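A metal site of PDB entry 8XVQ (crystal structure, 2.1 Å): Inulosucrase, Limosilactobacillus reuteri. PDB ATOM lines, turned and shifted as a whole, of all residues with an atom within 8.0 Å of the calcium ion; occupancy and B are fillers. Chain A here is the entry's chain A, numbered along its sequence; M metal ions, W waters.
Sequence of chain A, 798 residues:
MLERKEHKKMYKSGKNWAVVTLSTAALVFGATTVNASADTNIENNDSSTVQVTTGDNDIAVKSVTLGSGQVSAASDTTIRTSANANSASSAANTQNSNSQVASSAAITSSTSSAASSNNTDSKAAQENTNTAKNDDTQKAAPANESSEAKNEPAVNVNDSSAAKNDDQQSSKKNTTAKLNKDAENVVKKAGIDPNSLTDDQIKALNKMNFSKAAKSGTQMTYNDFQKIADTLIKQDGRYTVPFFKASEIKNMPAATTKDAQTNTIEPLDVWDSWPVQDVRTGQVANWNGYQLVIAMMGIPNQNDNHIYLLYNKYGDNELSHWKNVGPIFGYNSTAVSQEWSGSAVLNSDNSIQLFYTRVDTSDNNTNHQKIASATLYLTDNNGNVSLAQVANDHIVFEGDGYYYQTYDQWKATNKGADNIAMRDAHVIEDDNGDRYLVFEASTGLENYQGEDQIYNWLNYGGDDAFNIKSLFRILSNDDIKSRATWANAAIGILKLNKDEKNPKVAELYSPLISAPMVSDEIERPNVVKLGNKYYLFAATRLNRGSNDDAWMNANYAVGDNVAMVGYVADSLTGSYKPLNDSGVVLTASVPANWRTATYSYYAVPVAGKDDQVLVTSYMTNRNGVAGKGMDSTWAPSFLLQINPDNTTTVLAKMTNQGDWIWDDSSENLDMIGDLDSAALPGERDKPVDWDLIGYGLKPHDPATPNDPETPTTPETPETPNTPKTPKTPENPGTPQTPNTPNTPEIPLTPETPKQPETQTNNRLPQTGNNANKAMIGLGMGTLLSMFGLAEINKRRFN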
ATOM      1  N   GLN A 291      29.169  12.819  14.734  1.00  0.00           N
ATOM      2  CA  GLN A 291      28.168  13.442  13.866  1.00  0.00           C
ATOM      3  C   GLN A 291      27.922  14.877  14.375  1.00  0.00           C
ATOM      4  O   GLN A 291      27.935  15.125  15.578  1.00  0.00           O
ATOM      5  CB  GLN A 291      26.856  12.632  13.858  1.00  0.00           C
ATOM      6  CG  GLN A 291      26.293  12.398  15.239  1.00  0.00           C
ATOM      7  CD  GLN A 291      25.014  11.599  15.220  1.00  0.00           C
ATOM      8  OE1 GLN A 291      24.090  11.874  14.432  1.00  0.00           O
ATOM      9  NE2 GLN A 291      24.940  10.589  16.086  1.00  0.00           N
ATOM     10  N   LYS A 313      28.555  11.302  19.361  1.00  0.00           N
ATOM     11  CA  LYS A 313      29.340  10.220  18.782  1.00  0.00           C
ATOM     12  C   LYS A 313      28.580   9.704  17.559  1.00  0.00           C
ATOM     13  O   LYS A 313      27.355   9.528  17.617  1.00  0.00           O
ATOM     14  CB  LYS A 313      29.571   9.080  19.786  1.00  0.00           C
ATOM     15  CG  LYS A 313      30.689   9.324  20.795  1.00  0.00           C
ATOM     16  CD  LYS A 313      32.056   9.018  20.189  1.00  0.00           C
ATOM     17  CE  LYS A 313      33.212   9.651  20.953  1.00  0.00           C
ATOM     18  NZ  LYS A 313      34.300  10.075  20.024  1.00  0.00           N
ATOM     19  N   TYR A 314      29.299   9.492  16.473  1.00  0.00           N
ATOM     20  CA  TYR A 314      28.680   8.999  15.269  1.00  0.00           C
ATOM     21  C   TYR A 314      27.951   7.658  15.515  1.00  0.00           C
ATOM     22  O   TYR A 314      28.530   6.706  16.049  1.00  0.00           O
ATOM     23  CB  TYR A 314      29.722   8.854  14.161  1.00  0.00           C
ATOM     24  CG  TYR A 314      29.099   8.518  12.828  1.00  0.00           C
ATOM     25  CD1 TYR A 314      28.790   7.210  12.512  1.00  0.00           C
ATOM     26  CD2 TYR A 314      28.790   9.514  11.913  1.00  0.00           C
ATOM     27  CE1 TYR A 314      28.226   6.889  11.296  1.00  0.00           C
ATOM     28  CE2 TYR A 314      28.216   9.204  10.689  1.00  0.00           C
ATOM     29  CZ  TYR A 314      27.931   7.884  10.398  1.00  0.00           C
ATOM     30  OH  TYR A 314      27.364   7.526   9.207  1.00  0.00           O
ATOM     31  N   GLY A 315      26.669   7.627  15.158  1.00  0.00           N
ATOM     32  CA  GLY A 315      25.850   6.425  15.294  1.00  0.00           C
ATOM     33  C   GLY A 315      25.063   6.364  16.593  1.00  0.00           C
ATOM     34  O   GLY A 315      24.184   5.520  16.738  1.00  0.00           O
ATOM     35  N   ASP A 316      25.359   7.253  17.527  1.00  0.00           N
ATOM     36  CA  ASP A 316      24.716   7.242  18.829  1.00  0.00           C
ATOM     37  C   ASP A 316      23.259   7.657  18.676  1.00  0.00           C
ATOM     38  O   ASP A 316      22.963   8.638  18.011  1.00  0.00           O
ATOM     39  CB  ASP A 316      25.422   8.223  19.755  1.00  0.00           C
ATOM     40  CG  ASP A 316      24.778   8.304  21.113  1.00  0.00           C
ATOM     41  OD1 ASP A 316      23.692   8.908  21.249  1.00  0.00           O
ATOM     42  OD2 ASP A 316      25.401   7.782  22.068  1.00  0.00           O
ATOM     43  N   ASN A 317      22.364   6.928  19.331  1.00  0.00           N
ATOM     44  CA  ASN A 317      20.930   7.137  19.157  1.00  0.00           C
ATOM     45  C   ASN A 317      20.224   7.852  20.290  1.00  0.00           C
ATOM     46  O   ASN A 317      18.996   7.876  20.300  1.00  0.00           O
ATOM     47  CB  ASN A 317      20.239   5.796  18.930  1.00  0.00           C
ATOM     48  CG  ASN A 317      20.740   5.112  17.690  1.00  0.00           C
ATOM     49  OD1 ASN A 317      21.136   5.784  16.732  1.00  0.00           O
ATOM     50  ND2 ASN A 317      20.773   3.800  17.709  1.00  0.00           N
ATOM     51  N   GLU A 318      20.958   8.421  21.222  1.00  0.00           N
ATOM     52  CA  GLU A 318      20.325   9.011  22.396  1.00  0.00           C
ATOM     53  C   GLU A 318      20.223  10.516  22.245  1.00  0.00           C
ATOM     54  O   GLU A 318      21.227  11.200  22.054  1.00  0.00           O
ATOM     55  CB  GLU A 318      21.064   8.631  23.692  1.00  0.00           C
ATOM     56  CG  GLU A 318      21.223   7.126  23.930  1.00  0.00           C
ATOM     57  CD  GLU A 318      19.906   6.351  23.942  1.00  0.00           C
ATOM     58  OE1 GLU A 318      18.882   6.892  24.432  1.00  0.00           O
ATOM     59  OE2 GLU A 318      19.898   5.195  23.446  1.00  0.00           O
ATOM     60  N   LEU A 614      15.512   8.989   5.348  1.00  0.00           N
ATOM     61  CA  LEU A 614      15.118   9.187   6.755  1.00  0.00           C
ATOM     62  C   LEU A 614      14.609  10.631   6.935  1.00  0.00           C
ATOM     63  O   LEU A 614      15.369  11.590   6.753  1.00  0.00           O
ATOM     64  CB  LEU A 614      16.296   8.908   7.686  1.00  0.00           C
ATOM     65  CG  LEU A 614      15.977   8.968   9.187  1.00  0.00           C
ATOM     66  CD1 LEU A 614      15.108   7.787   9.579  1.00  0.00           C
ATOM     67  CD2 LEU A 614      17.254   9.025  10.027  1.00  0.00           C
ATOM     68  N   THR A 655      12.644   6.021  14.672  1.00  0.00           N
ATOM     69  CA  THR A 655      13.812   6.044  15.538  1.00  0.00           C
ATOM     70  C   THR A 655      13.469   6.706  16.868  1.00  0.00           C
ATOM     71  O   THR A 655      12.324   7.147  17.068  1.00  0.00           O
ATOM     72  CB  THR A 655      14.957   6.866  14.914  1.00  0.00           C
ATOM     73  OG1 THR A 655      14.568   8.245  14.862  1.00  0.00           O
ATOM     74  CG2 THR A 655      15.276   6.368  13.535  1.00  0.00           C
ATOM     75  N   ASN A 656      14.463   6.783  17.752  1.00  0.00           N
ATOM     76  CA  ASN A 656      14.461   7.719  18.879  1.00  0.00           C
ATOM     77  C   ASN A 656      14.380   9.154  18.381  1.00  0.00           C
ATOM     78  O   ASN A 656      14.658   9.425  17.211  1.00  0.00           O
ATOM     79  CB  ASN A 656      15.761   7.643  19.702  1.00  0.00           C
ATOM     80  CG  ASN A 656      15.886   6.361  20.510  1.00  0.00           C
ATOM     81  OD1 ASN A 656      14.909   5.713  20.836  1.00  0.00           O
ATOM     82  ND2 ASN A 656      17.117   6.004  20.832  1.00  0.00           N
ATOM     83  N   GLY A 658      15.571  12.588  17.401  1.00  0.00           N
ATOM     84  CA  GLY A 658      16.803  13.269  17.066  1.00  0.00           C
ATOM     85  C   GLY A 658      17.844  12.390  16.432  1.00  0.00           C
ATOM     86  O   GLY A 658      19.027  12.714  16.459  1.00  0.00           O
ATOM     87  N   ASP A 659      17.397  11.276  15.826  1.00  0.00           N
ATOM     88  CA  ASP A 659      18.293  10.350  15.147  1.00  0.00           C
ATOM     89  C   ASP A 659      18.431  10.749  13.662  1.00  0.00           C
ATOM     90  O   ASP A 659      17.422  10.814  12.929  1.00  0.00           O
ATOM     91  CB  ASP A 659      17.722   8.938  15.298  1.00  0.00           C
ATOM     92  CG  ASP A 659      18.687   7.845  14.906  1.00  0.00           C
ATOM     93  OD1 ASP A 659      19.683   8.101  14.229  1.00  0.00           O
ATOM     94  OD2 ASP A 659      18.403   6.679  15.262  1.00  0.00           O
ATOM     95  N   TRP A 660      19.659  11.011  13.229  1.00  0.00           N
ATOM     96  CA  TRP A 660      19.947  11.468  11.872  1.00  0.00           C
ATOM     97  C   TRP A 660      20.546  10.372  10.994  1.00  0.00           C
ATOM     98  O   TRP A 660      20.777  10.600   9.810  1.00  0.00           O
ATOM     99  CB  TRP A 660      20.934  12.638  11.906  1.00  0.00           C
ATOM    100  CG  TRP A 660      20.378  13.841  12.604  1.00  0.00           C
ATOM    101  CD1 TRP A 660      20.347  14.069  13.938  1.00  0.00           C
ATOM    102  CD2 TRP A 660      19.774  14.983  11.988  1.00  0.00           C
ATOM    103  NE1 TRP A 660      19.753  15.265  14.207  1.00  0.00           N
ATOM    104  CE2 TRP A 660      19.387  15.859  13.030  1.00  0.00           C
ATOM    105  CE3 TRP A 660      19.495  15.338  10.668  1.00  0.00           C
ATOM    106  CZ2 TRP A 660      18.746  17.069  12.787  1.00  0.00           C
ATOM    107  CZ3 TRP A 660      18.860  16.558  10.433  1.00  0.00           C
ATOM    108  CH2 TRP A 660      18.500  17.399  11.490  1.00  0.00           C
ATOM    109  N   ILE A 661      20.810   9.199  11.580  1.00  0.00           N
ATOM    110  CA  ILE A 661      21.527   8.137  10.894  1.00  0.00           C
ATOM    111  C   ILE A 661      20.762   6.838  11.085  1.00  0.00           C
ATOM    112  O   ILE A 661      20.836   6.232  12.155  1.00  0.00           O
ATOM    113  CB  ILE A 661      22.959   7.940  11.467  1.00  0.00           C
ATOM    114  CG1 ILE A 661      23.759   9.254  11.421  1.00  0.00           C
ATOM    115  CG2 ILE A 661      23.709   6.847  10.699  1.00  0.00           C
ATOM    116  CD1 ILE A 661      24.930   9.280  12.370  1.00  0.00           C
ATOM    117  N   TRP A 662      20.046   6.385  10.065  1.00  0.00           N
ATOM    118  CA  TRP A 662      19.309   5.151  10.179  1.00  0.00           C
ATOM    119  C   TRP A 662      20.264   3.976   9.985  1.00  0.00           C
ATOM    120  O   TRP A 662      21.100   3.987   9.096  1.00  0.00           O
ATOM    121  CB  TRP A 662      18.190   5.048   9.147  1.00  0.00           C
ATOM    122  CG  TRP A 662      17.555   3.678   9.146  1.00  0.00           C
ATOM    123  CD1 TRP A 662      17.976   2.577   8.440  1.00  0.00           C
ATOM    124  CD2 TRP A 662      16.442   3.237   9.928  1.00  0.00           C
ATOM    125  NE1 TRP A 662      17.186   1.499   8.745  1.00  0.00           N
ATOM    126  CE2 TRP A 662      16.234   1.871   9.648  1.00  0.00           C
ATOM    127  CE3 TRP A 662      15.597   3.876  10.837  1.00  0.00           C
ATOM    128  CZ2 TRP A 662      15.218   1.136  10.225  1.00  0.00           C
ATOM    129  CZ3 TRP A 662      14.583   3.142  11.424  1.00  0.00           C
ATOM    130  CH2 TRP A 662      14.400   1.776  11.116  1.00  0.00           C
ATOM    131  N   ASP A 663      20.124   2.970  10.840  1.00  0.00           N
ATOM    132  CA  ASP A 663      20.695   1.627  10.591  1.00  0.00           C
ATOM    133  C   ASP A 663      19.779   0.628  11.286  1.00  0.00           C
ATOM    134  O   ASP A 663      18.750   1.018  11.864  1.00  0.00           O
ATOM    135  CB  ASP A 663      22.157   1.539  11.050  1.00  0.00           C
ATOM    136  CG  ASP A 663      22.359   2.017  12.469  1.00  0.00           C
ATOM    137  OD1 ASP A 663      21.507   1.737  13.334  1.00  0.00           O
ATOM    138  OD2 ASP A 663      23.380   2.685  12.726  1.00  0.00           O
ATOM    139  N   ASP A 664      20.136  -0.654  11.245  1.00  0.00           N
ATOM    140  CA  ASP A 664      19.322  -1.709  11.860  1.00  0.00           C
ATOM    141  C   ASP A 664      19.087  -1.492  13.353  1.00  0.00           C
ATOM    142  O   ASP A 664      17.996  -1.731  13.868  1.00  0.00           O
ATOM    143  CB  ASP A 664      19.986  -3.077  11.658  1.00  0.00           C
ATOM    144  CG  ASP A 664      19.884  -3.569  10.230  1.00  0.00           C
ATOM    145  OD1 ASP A 664      19.027  -3.077   9.465  1.00  0.00           O
ATOM    146  OD2 ASP A 664      20.678  -4.471   9.885  1.00  0.00           O
ATOM    147  N   SER A 665      20.113  -1.009  14.034  1.00  0.00           N
ATOM    148  CA  SER A 665      20.035  -0.827  15.471  1.00  0.00           C
ATOM    149  C   SER A 665      19.279   0.451  15.888  1.00  0.00           C
ATOM    150  O   SER A 665      19.036   0.651  17.069  1.00  0.00           O
ATOM    151  CB  SER A 665      21.438  -0.796  16.064  1.00  0.00           C
ATOM    152  OG  SER A 665      22.121   0.375  15.667  1.00  0.00           O
ATOM    153  N   SER A 666      18.944   1.322  14.929  1.00  0.00           N
ATOM    154  CA  SER A 666      18.332   2.608  15.279  1.00  0.00           C
ATOM    155  C   SER A 666      16.829   2.519  15.489  1.00  0.00           C
ATOM    156  O   SER A 666      16.233   3.441  16.055  1.00  0.00           O
ATOM    157  CB  SER A 666      18.621   3.656  14.186  1.00  0.00           C
ATOM    158  OG  SER A 666      19.995   3.974  14.059  1.00  0.00           O
ATOM    159  N   GLU A 667      16.189   1.442  15.034  1.00  0.00           N
ATOM    160  CA  GLU A 667      14.733   1.343  15.114  1.00  0.00           C
ATOM    161  C   GLU A 667      14.211   1.261  16.532  1.00  0.00           C
ATOM    162  O   GLU A 667      14.730   0.511  17.340  1.00  0.00           O
ATOM    163  CB  GLU A 667      14.227   0.136  14.356  1.00  0.00           C
ATOM    164  CG  GLU A 667      12.708   0.035  14.330  1.00  0.00           C
ATOM    165  CD  GLU A 667      12.211  -0.865  13.228  1.00  0.00           C
ATOM    166  OE1 GLU A 667      12.689  -2.007  13.137  1.00  0.00           O
ATOM    167  OE2 GLU A 667      11.344  -0.435  12.451  1.00  0.00           O
HETATM  168 CA    CA M   1      20.889   6.105  14.460  1.00  0.00          CA
HETATM  169  O   HOH W   1      22.367   7.793  15.075  1.00  0.00           O
HETATM  170  O   HOH W   2      22.870   4.896  14.352  1.00  0.00           O
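Water W2 lies within hydrogen-bond range of OD2 of Asp 663 and O of Gly 315.
The calcium ion is bound by the side-chain amide oxygen (OD1) of Asn 317 (2.3 Å), the backbone carbonyl oxygen (O) of Ile 661 (2.3 Å), water W2 (2.3 Å), water W1 (2.3 Å), the side-chain carboxylate (OD1) of Asp 659 (2.3 Å), the side-chain hydroxyl (OG) of Ser 666 (2.3 Å) and the side-chain carboxylate (OD2) of Asp 659 (2.7 Å). The calcium ion has seven donor atoms within binding distance.
The backbone carbonyl oxygen (O) of Gly 315 sits close to the side-chain amide oxygen (OD1) of Asn 317, 3.1 Å away. OD1 of Asp 663 is in hydrogen-bond range of N of Ser 666 (3.0 Å). O of Asn 317 is in hydrogen-bond range of ND2 of Asn 656.
Four residues have an atom within 4 Å of the calcium ion: Asn 317, Asp 659, Ile 661 and Ser 666. The nearest printed residue that does not touch the calcium ion is Gly 315 (4.05 Å).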
